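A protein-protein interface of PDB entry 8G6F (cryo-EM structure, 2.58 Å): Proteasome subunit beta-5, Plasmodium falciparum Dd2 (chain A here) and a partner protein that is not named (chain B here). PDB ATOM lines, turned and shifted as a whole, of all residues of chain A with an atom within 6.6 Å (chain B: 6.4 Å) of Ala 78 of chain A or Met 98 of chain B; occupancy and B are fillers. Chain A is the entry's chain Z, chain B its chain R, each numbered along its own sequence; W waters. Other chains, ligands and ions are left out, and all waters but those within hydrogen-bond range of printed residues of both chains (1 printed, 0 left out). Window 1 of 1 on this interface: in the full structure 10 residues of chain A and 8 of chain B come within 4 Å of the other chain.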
ATOM      1  N   LEU A  59       0.665 -23.346  -1.257  1.00  0.00           N
ATOM      2  CA  LEU A  59       0.791 -22.950  -2.653  1.00  0.00           C
ATOM      3  C   LEU A  59       1.044 -24.160  -3.541  1.00  0.00           C
ATOM      4  O   LEU A  59       0.528 -24.234  -4.660  1.00  0.00           O
ATOM      5  CB  LEU A  59       1.914 -21.926  -2.804  1.00  0.00           C
ATOM      6  CG  LEU A  59       2.182 -21.409  -4.218  1.00  0.00           C
ATOM      7  CD1 LEU A  59       1.077 -20.471  -4.655  1.00  0.00           C
ATOM      8  CD2 LEU A  59       3.525 -20.722  -4.291  1.00  0.00           C
ATOM      9  N   ILE A  63      -1.250 -25.294  -6.675  1.00  0.00           N
ATOM     10  CA  ILE A  63      -0.666 -25.437  -8.002  1.00  0.00           C
ATOM     11  C   ILE A  63      -0.876 -26.848  -8.532  1.00  0.00           C
ATOM     12  O   ILE A  63      -1.113 -27.042  -9.727  1.00  0.00           O
ATOM     13  CB  ILE A  63       0.823 -25.060  -7.959  1.00  0.00           C
ATOM     14  CG1 ILE A  63       0.961 -23.548  -7.806  1.00  0.00           C
ATOM     15  CG2 ILE A  63       1.526 -25.554  -9.208  1.00  0.00           C
ATOM     16  CD1 ILE A  63       2.350 -23.092  -7.491  1.00  0.00           C
ATOM     17  N   TYR A  66      -4.460 -27.069  -9.701  1.00  0.00           N
ATOM     18  CA  TYR A  66      -4.624 -26.277 -10.916  1.00  0.00           C
ATOM     19  C   TYR A  66      -4.052 -27.004 -12.124  1.00  0.00           C
ATOM     20  O   TYR A  66      -4.680 -27.060 -13.189  1.00  0.00           O
ATOM     21  CB  TYR A  66      -3.949 -24.915 -10.741  1.00  0.00           C
ATOM     22  CG  TYR A  66      -3.733 -24.172 -12.038  1.00  0.00           C
ATOM     23  CD1 TYR A  66      -4.708 -23.328 -12.546  1.00  0.00           C
ATOM     24  CD2 TYR A  66      -2.557 -24.317 -12.757  1.00  0.00           C
ATOM     25  CE1 TYR A  66      -4.519 -22.659 -13.728  1.00  0.00           C
ATOM     26  CE2 TYR A  66      -2.363 -23.652 -13.941  1.00  0.00           C
ATOM     27  CZ  TYR A  66      -3.346 -22.822 -14.421  1.00  0.00           C
ATOM     28  OH  TYR A  66      -3.151 -22.152 -15.604  1.00  0.00           O
ATOM     29  N   GLU A  72      -1.950 -28.036 -17.764  1.00  0.00           N
ATOM     30  CA  GLU A  72      -0.872 -27.139 -18.138  1.00  0.00           C
ATOM     31  C   GLU A  72      -0.110 -26.749 -16.886  1.00  0.00           C
ATOM     32  O   GLU A  72      -0.642 -26.789 -15.777  1.00  0.00           O
ATOM     33  CB  GLU A  72      -1.389 -25.885 -18.854  1.00  0.00           C
ATOM     34  CG  GLU A  72      -2.146 -24.917 -17.961  1.00  0.00           C
ATOM     35  CD  GLU A  72      -2.767 -23.778 -18.742  1.00  0.00           C
ATOM     36  OE1 GLU A  72      -2.366 -23.564 -19.906  1.00  0.00           O
ATOM     37  OE2 GLU A  72      -3.654 -23.092 -18.195  1.00  0.00           O
ATOM     38  N   ILE A  74       1.611 -24.215 -14.315  1.00  0.00           N
ATOM     39  CA  ILE A  74       1.329 -22.857 -13.876  1.00  0.00           C
ATOM     40  C   ILE A  74       2.552 -21.974 -14.104  1.00  0.00           C
ATOM     41  O   ILE A  74       3.696 -22.435 -14.149  1.00  0.00           O
ATOM     42  CB  ILE A  74       0.896 -22.836 -12.401  1.00  0.00           C
ATOM     43  CG1 ILE A  74       0.016 -21.617 -12.128  1.00  0.00           C
ATOM     44  CG2 ILE A  74       2.110 -22.837 -11.490  1.00  0.00           C
ATOM     45  CD1 ILE A  74      -0.343 -21.432 -10.686  1.00  0.00           C
ATOM     46  N   SER A  75       2.297 -20.680 -14.252  1.00  0.00           N
ATOM     47  CA  SER A  75       3.355 -19.709 -14.465  1.00  0.00           C
ATOM     48  C   SER A  75       3.835 -19.140 -13.134  1.00  0.00           C
ATOM     49  O   SER A  75       3.110 -19.117 -12.135  1.00  0.00           O
ATOM     50  CB  SER A  75       2.878 -18.582 -15.378  1.00  0.00           C
ATOM     51  OG  SER A  75       2.074 -17.658 -14.674  1.00  0.00           O
ATOM     52  N   VAL A  76       5.086 -18.681 -13.135  1.00  0.00           N
ATOM     53  CA  VAL A  76       5.663 -18.110 -11.924  1.00  0.00           C
ATOM     54  C   VAL A  76       4.873 -16.884 -11.495  1.00  0.00           C
ATOM     55  O   VAL A  76       4.673 -16.644 -10.302  1.00  0.00           O
ATOM     56  CB  VAL A  76       7.151 -17.778 -12.141  1.00  0.00           C
ATOM     57  CG1 VAL A  76       7.800 -17.385 -10.832  1.00  0.00           C
ATOM     58  CG2 VAL A  76       7.877 -18.957 -12.756  1.00  0.00           C
ATOM     59  N   ARG A  77       4.409 -16.091 -12.461  1.00  0.00           N
ATOM     60  CA  ARG A  77       3.620 -14.910 -12.133  1.00  0.00           C
ATOM     61  C   ARG A  77       2.318 -15.289 -11.441  1.00  0.00           C
ATOM     62  O   ARG A  77       1.929 -14.662 -10.450  1.00  0.00           O
ATOM     63  CB  ARG A  77       3.342 -14.109 -13.402  1.00  0.00           C
ATOM     64  CG  ARG A  77       2.298 -13.022 -13.248  1.00  0.00           C
ATOM     65  CD  ARG A  77       2.097 -12.264 -14.539  1.00  0.00           C
ATOM     66  NE  ARG A  77       3.339 -11.697 -15.044  1.00  0.00           N
ATOM     67  CZ  ARG A  77       3.890 -10.577 -14.598  1.00  0.00           C
ATOM     68  NH1 ARG A  77       3.329  -9.866 -13.635  1.00  0.00           N
ATOM     69  NH2 ARG A  77       5.034 -10.160 -15.131  1.00  0.00           N
ATOM     70  N   ALA A  78       1.626 -16.307 -11.953  1.00  0.00           N
ATOM     71  CA  ALA A  78       0.374 -16.732 -11.341  1.00  0.00           C
ATOM     72  C   ALA A  78       0.604 -17.297  -9.947  1.00  0.00           C
ATOM     73  O   ALA A  78      -0.175 -17.025  -9.025  1.00  0.00           O
ATOM     74  CB  ALA A  78      -0.316 -17.762 -12.225  1.00  0.00           C
ATOM     75  N   ALA A  79       1.661 -18.091  -9.774  1.00  0.00           N
ATOM     76  CA  ALA A  79       1.963 -18.630  -8.453  1.00  0.00           C
ATOM     77  C   ALA A  79       2.286 -17.514  -7.469  1.00  0.00           C
ATOM     78  O   ALA A  79       1.844 -17.542  -6.312  1.00  0.00           O
ATOM     79  CB  ALA A  79       3.122 -19.618  -8.548  1.00  0.00           C
ATOM     80  N   SER A  80       3.052 -16.517  -7.912  1.00  0.00           N
ATOM     81  CA  SER A  80       3.374 -15.388  -7.050  1.00  0.00           C
ATOM     82  C   SER A  80       2.126 -14.602  -6.685  1.00  0.00           C
ATOM     83  O   SER A  80       1.983 -14.147  -5.548  1.00  0.00           O
ATOM     84  CB  SER A  80       4.392 -14.485  -7.739  1.00  0.00           C
ATOM     85  OG  SER A  80       5.366 -15.252  -8.416  1.00  0.00           O
ATOM     86  N   THR A  81       1.216 -14.417  -7.640  1.00  0.00           N
ATOM     87  CA  THR A  81      -0.025 -13.715  -7.339  1.00  0.00           C
ATOM     88  C   THR A  81      -0.859 -14.481  -6.320  1.00  0.00           C
ATOM     89  O   THR A  81      -1.403 -13.888  -5.382  1.00  0.00           O
ATOM     90  CB  THR A  81      -0.824 -13.493  -8.618  1.00  0.00           C
ATOM     91  OG1 THR A  81       0.028 -12.930  -9.621  1.00  0.00           O
ATOM     92  CG2 THR A  81      -1.976 -12.552  -8.360  1.00  0.00           C
ATOM     93  N   ILE A  82      -0.971 -15.799  -6.485  1.00  0.00           N
ATOM     94  CA  ILE A  82      -1.729 -16.598  -5.527  1.00  0.00           C
ATOM     95  C   ILE A  82      -1.129 -16.455  -4.135  1.00  0.00           C
ATOM     96  O   ILE A  82      -1.838 -16.200  -3.151  1.00  0.00           O
ATOM     97  CB  ILE A  82      -1.768 -18.071  -5.970  1.00  0.00           C
ATOM     98  CG1 ILE A  82      -2.598 -18.229  -7.242  1.00  0.00           C
ATOM     99  CG2 ILE A  82      -2.336 -18.938  -4.865  1.00  0.00           C
ATOM    100  CD1 ILE A  82      -2.333 -19.512  -7.983  1.00  0.00           C
ATOM    101  N   LEU A  83       0.193 -16.606  -4.037  1.00  0.00           N
ATOM    102  CA  LEU A  83       0.849 -16.531  -2.739  1.00  0.00           C
ATOM    103  C   LEU A  83       0.683 -15.153  -2.111  1.00  0.00           C
ATOM    104  O   LEU A  83       0.417 -15.041  -0.910  1.00  0.00           O
ATOM    105  CB  LEU A  83       2.326 -16.879  -2.888  1.00  0.00           C
ATOM    106  CG  LEU A  83       3.154 -16.994  -1.608  1.00  0.00           C
ATOM    107  CD1 LEU A  83       2.635 -18.088  -0.691  1.00  0.00           C
ATOM    108  CD2 LEU A  83       4.600 -17.242  -1.972  1.00  0.00           C
ATOM    109  N   ASN A  85      -1.698 -12.875  -2.648  1.00  0.00           N
ATOM    110  CA  ASN A  85      -3.070 -12.663  -2.201  1.00  0.00           C
ATOM    111  C   ASN A  85      -3.344 -13.409  -0.903  1.00  0.00           C
ATOM    112  O   ASN A  85      -3.945 -12.856   0.030  1.00  0.00           O
ATOM    113  CB  ASN A  85      -4.050 -13.098  -3.287  1.00  0.00           C
ATOM    114  CG  ASN A  85      -4.058 -12.161  -4.472  1.00  0.00           C
ATOM    115  OD1 ASN A  85      -3.392 -11.131  -4.467  1.00  0.00           O
ATOM    116  ND2 ASN A  85      -4.814 -12.515  -5.498  1.00  0.00           N
ATOM    117  N   PHE A 112      10.056 -13.536  -8.946  1.00  0.00           N
ATOM    118  CA  PHE A 112       9.208 -12.624  -8.196  1.00  0.00           C
ATOM    119  C   PHE A 112       9.562 -12.685  -6.720  1.00  0.00           C
ATOM    120  O   PHE A 112       9.792 -13.764  -6.169  1.00  0.00           O
ATOM    121  CB  PHE A 112       7.722 -12.960  -8.372  1.00  0.00           C
ATOM    122  CG  PHE A 112       7.190 -12.667  -9.740  1.00  0.00           C
ATOM    123  CD1 PHE A 112       7.431 -13.531 -10.792  1.00  0.00           C
ATOM    124  CD2 PHE A 112       6.438 -11.535  -9.976  1.00  0.00           C
ATOM    125  CE1 PHE A 112       6.943 -13.266 -12.043  1.00  0.00           C
ATOM    126  CE2 PHE A 112       5.945 -11.273 -11.230  1.00  0.00           C
ATOM    127  CZ  PHE A 112       6.202 -12.139 -12.264  1.00  0.00           C
ATOM    128  N   LYS A 120       4.554  -8.021  -4.333  1.00  0.00           N
ATOM    129  CA  LYS A 120       4.886  -8.929  -5.427  1.00  0.00           C
ATOM    130  C   LYS A 120       5.656  -8.109  -6.454  1.00  0.00           C
ATOM    131  O   LYS A 120       5.057  -7.362  -7.229  1.00  0.00           O
ATOM    132  CB  LYS A 120       3.638  -9.560  -6.027  1.00  0.00           C
ATOM    133  CG  LYS A 120       3.914 -10.440  -7.232  1.00  0.00           C
ATOM    134  CD  LYS A 120       2.645 -11.018  -7.811  1.00  0.00           C
ATOM    135  CE  LYS A 120       1.785  -9.954  -8.459  1.00  0.00           C
ATOM    136  NZ  LYS A 120       1.636 -10.176  -9.915  1.00  0.00           N
ATOM    137  N   ARG B  93     -12.533 -12.220 -12.142  1.00  0.00           N
ATOM    138  CA  ARG B  93     -12.045 -12.854 -10.922  1.00  0.00           C
ATOM    139  C   ARG B  93     -10.800 -13.686 -11.194  1.00  0.00           C
ATOM    140  O   ARG B  93      -9.849 -13.670 -10.405  1.00  0.00           O
ATOM    141  CB  ARG B  93     -13.142 -13.719 -10.308  1.00  0.00           C
ATOM    142  CG  ARG B  93     -12.861 -14.155  -8.883  1.00  0.00           C
ATOM    143  CD  ARG B  93     -13.748 -15.314  -8.459  1.00  0.00           C
ATOM    144  NE  ARG B  93     -14.968 -14.860  -7.799  1.00  0.00           N
ATOM    145  CZ  ARG B  93     -16.192 -14.944  -8.306  1.00  0.00           C
ATOM    146  NH1 ARG B  93     -16.416 -15.455  -9.507  1.00  0.00           N
ATOM    147  NH2 ARG B  93     -17.221 -14.503  -7.588  1.00  0.00           N
ATOM    148  N   TYR B  94     -10.787 -14.422 -12.304  1.00  0.00           N
ATOM    149  CA  TYR B  94      -9.593 -15.162 -12.686  1.00  0.00           C
ATOM    150  C   TYR B  94      -8.433 -14.217 -12.946  1.00  0.00           C
ATOM    151  O   TYR B  94      -7.300 -14.486 -12.534  1.00  0.00           O
ATOM    152  CB  TYR B  94      -9.881 -16.012 -13.921  1.00  0.00           C
ATOM    153  CG  TYR B  94      -8.720 -16.859 -14.386  1.00  0.00           C
ATOM    154  CD1 TYR B  94      -7.661 -16.297 -15.080  1.00  0.00           C
ATOM    155  CD2 TYR B  94      -8.687 -18.220 -14.138  1.00  0.00           C
ATOM    156  CE1 TYR B  94      -6.600 -17.063 -15.504  1.00  0.00           C
ATOM    157  CE2 TYR B  94      -7.629 -18.994 -14.561  1.00  0.00           C
ATOM    158  CZ  TYR B  94      -6.592 -18.410 -15.246  1.00  0.00           C
ATOM    159  OH  TYR B  94      -5.537 -19.176 -15.671  1.00  0.00           O
ATOM    160  N   TYR B  95      -8.688 -13.109 -13.642  1.00  0.00           N
ATOM    161  CA  TYR B  95      -7.616 -12.151 -13.882  1.00  0.00           C
ATOM    162  C   TYR B  95      -7.065 -11.615 -12.568  1.00  0.00           C
ATOM    163  O   TYR B  95      -5.849 -11.521 -12.388  1.00  0.00           O
ATOM    164  CB  TYR B  95      -8.120 -11.008 -14.759  1.00  0.00           C
ATOM    165  CG  TYR B  95      -7.053 -10.357 -15.606  1.00  0.00           C
ATOM    166  CD1 TYR B  95      -5.729 -10.331 -15.200  1.00  0.00           C
ATOM    167  CD2 TYR B  95      -7.372  -9.756 -16.810  1.00  0.00           C
ATOM    168  CE1 TYR B  95      -4.762  -9.739 -15.967  1.00  0.00           C
ATOM    169  CE2 TYR B  95      -6.406  -9.161 -17.584  1.00  0.00           C
ATOM    170  CZ  TYR B  95      -5.104  -9.157 -17.157  1.00  0.00           C
ATOM    171  OH  TYR B  95      -4.140  -8.559 -17.929  1.00  0.00           O
ATOM    172  N   LEU B  96      -7.945 -11.280 -11.629  1.00  0.00           N
ATOM    173  CA  LEU B  96      -7.494 -10.768 -10.342  1.00  0.00           C
ATOM    174  C   LEU B  96      -6.687 -11.810  -9.577  1.00  0.00           C
ATOM    175  O   LEU B  96      -5.699 -11.476  -8.917  1.00  0.00           O
ATOM    176  CB  LEU B  96      -8.698 -10.314  -9.521  1.00  0.00           C
ATOM    177  CG  LEU B  96      -8.420  -9.471  -8.279  1.00  0.00           C
ATOM    178  CD1 LEU B  96      -7.719  -8.179  -8.637  1.00  0.00           C
ATOM    179  CD2 LEU B  96      -9.716  -9.185  -7.555  1.00  0.00           C
ATOM    180  N   ASN B  97      -7.095 -13.076  -9.645  1.00  0.00           N
ATOM    181  CA  ASN B  97      -6.464 -14.109  -8.834  1.00  0.00           C
ATOM    182  C   ASN B  97      -5.179 -14.655  -9.438  1.00  0.00           C
ATOM    183  O   ASN B  97      -4.337 -15.167  -8.693  1.00  0.00           O
ATOM    184  CB  ASN B  97      -7.442 -15.260  -8.605  1.00  0.00           C
ATOM    185  CG  ASN B  97      -8.360 -15.014  -7.429  1.00  0.00           C
ATOM    186  OD1 ASN B  97      -7.920 -14.591  -6.362  1.00  0.00           O
ATOM    187  ND2 ASN B  97      -9.645 -15.272  -7.618  1.00  0.00           N
ATOM    188  N   MET B  98      -5.003 -14.570 -10.756  1.00  0.00           N
ATOM    189  CA  MET B  98      -3.849 -15.164 -11.412  1.00  0.00           C
ATOM    190  C   MET B  98      -2.944 -14.164 -12.110  1.00  0.00           C
ATOM    191  O   MET B  98      -1.849 -14.547 -12.533  1.00  0.00           O
ATOM    192  CB  MET B  98      -4.304 -16.209 -12.442  1.00  0.00           C
ATOM    193  CG  MET B  98      -5.143 -17.328 -11.858  1.00  0.00           C
ATOM    194  SD  MET B  98      -4.161 -18.728 -11.304  1.00  0.00           S
ATOM    195  CE  MET B  98      -3.555 -19.358 -12.860  1.00  0.00           C
ATOM    196  N   ASP B  99      -3.351 -12.906 -12.239  1.00  0.00           N
ATOM    197  CA  ASP B  99      -2.589 -11.883 -12.948  1.00  0.00           C
ATOM    198  C   ASP B  99      -2.450 -12.191 -14.433  1.00  0.00           C
ATOM    199  O   ASP B  99      -1.544 -11.679 -15.092  1.00  0.00           O
ATOM    200  CB  ASP B  99      -1.207 -11.694 -12.320  1.00  0.00           C
ATOM    201  CG  ASP B  99      -0.700 -10.275 -12.448  1.00  0.00           C
ATOM    202  OD1 ASP B  99      -1.383  -9.450 -13.087  1.00  0.00           O
ATOM    203  OD2 ASP B  99       0.387  -9.982 -11.911  1.00  0.00           O
ATOM    204  N   GLU B 100      -3.329 -13.025 -14.976  1.00  0.00           N
ATOM    205  CA  GLU B 100      -3.341 -13.352 -16.391  1.00  0.00           C
ATOM    206  C   GLU B 100      -4.782 -13.423 -16.866  1.00  0.00           C
ATOM    207  O   GLU B 100      -5.678 -13.746 -16.080  1.00  0.00           O
ATOM    208  CB  GLU B 100      -2.647 -14.693 -16.666  1.00  0.00           C
ATOM    209  CG  GLU B 100      -1.155 -14.678 -16.398  1.00  0.00           C
ATOM    210  CD  GLU B 100      -0.617 -16.038 -16.023  1.00  0.00           C
ATOM    211  OE1 GLU B 100      -1.354 -17.034 -16.176  1.00  0.00           O
ATOM    212  OE2 GLU B 100       0.543 -16.112 -15.568  1.00  0.00           O
HETATM  213  O   HOH W   1      -0.843 -19.750 -15.461  1.00  0.00           O
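Among the printed residues, pairs that only touch across the chains: Tyr 66 of chain A with Tyr 94 of chain B, Tyr 66 of chain A with Met 98 of chain B, Ala 78 of chain A with Met 98 of chain B, Ala 78 of chain A with Glu 100 of chain B, Thr 81 of chain A with Leu 96 of chain B, Thr 81 of chain A with Asn 97 of chain B, Thr 81 of chain A with Met 98 of chain B, Thr 81 of chain A with Asp 99 of chain B, Ile 82 of chain A with Asn 97 of chain B, Ile 82 of chain A with Met 98 of chain B, Asn 85 of chain A with Leu 96 of chain B and Asn 85 of chain A with Asn 97 of chain B.
Printed residues of chain A that touch a printed residue of chain B: Tyr 66, Ser 75, Arg 77, Ala 78, Thr 81, Ile 82, Asn 85 and Lys 120.
Hydrophobic or aromatic side chains of chain A that line the printed part of chain B: Tyr 66, Ala 78 and Ile 82.
Of the 8 printed residues of chain B, 6 touch a printed residue of chain A.
Among the printed residues, Asp or Glu carboxylates within 4 Å of a Lys or Arg side-chain nitrogen of the other chain: Arg 77 of chain A with Asp 99 of chain B (3.4 Å) and Lys 120 of chain A with Asp 99 of chain B (2.4 Å).
Water W1 lies within hydrogen-bond range of OE1 of Glu 100 of chain B, OH of Tyr 66 of chain A and N of Ser 75 of chain A.
Ala 78 of chain A touches just these residues of chain B: Met 98 and Glu 100.
Met 98 of chain B touches just these residues of chain A: Tyr 66, Ala 78, Thr 81 and Ile 82.
Printed residues of chain A within 4 Å of Tyr 94 of chain B: Tyr 66 (3.8 Å).
Of the printed residues of chain B, Tyr 66 of chain A touches Tyr 94 and Met 98.
Of the printed residues of chain A, Asn 97 of chain B touches Thr 81 (3.5 Å), Ile 82 (3.8 Å) and Asn 85 (3.8 Å).
Of the printed residues of chain B, Lys 120 of chain A touches Asp 99.
Val 76 of chain A touches none of the printed residues of chain B.
The nearest residue of chain B that does not touch Ala 78 of chain A is Asn 97 of chain B (4.6 Å).
The nearest printed residue of chain A that does not touch Met 98 of chain B is Ile 74 of chain A (4.3 Å).
The side-chain amide nitrogen of Asn 97 of chain B sits at hydrogen-bond distance from the backbone carbonyl oxygen of Arg 93 of chain B, at 3.2 Å.
OH of Tyr 66 of chain A is in hydrogen-bond range of OE2 of Glu 72 of chain A (2.8 Å).
The backbone carbonyl oxygen of Arg 77 of chain A lies within hydrogen-bond range of the side-chain hydroxyl of Thr 81 of chain A, at 2.7 Å.
The backbone NH (N) of Ala 78 of chain A lies within hydrogen-bond range of the side-chain hydroxyl (OG) of Ser 75 of chain A, at 3.1 Å.
The side-chain hydroxyl (OG1) of Thr 81 of chain A is in hydrogen-bond range of the side-chain amino group (NZ) of Lys 120 of chain A.
NZ of Lys 120 of chain A sits close to OD2 of Asp 99 of chain B (2.4 Å).
OE2 of Glu 100 of chain B sits close to OG of Ser 75 of chain A (2.4 Å).
OD2 of Asp 99 of chain B lies within salt-bridge range of NH1 of Arg 77 of chain A (3.4 Å).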
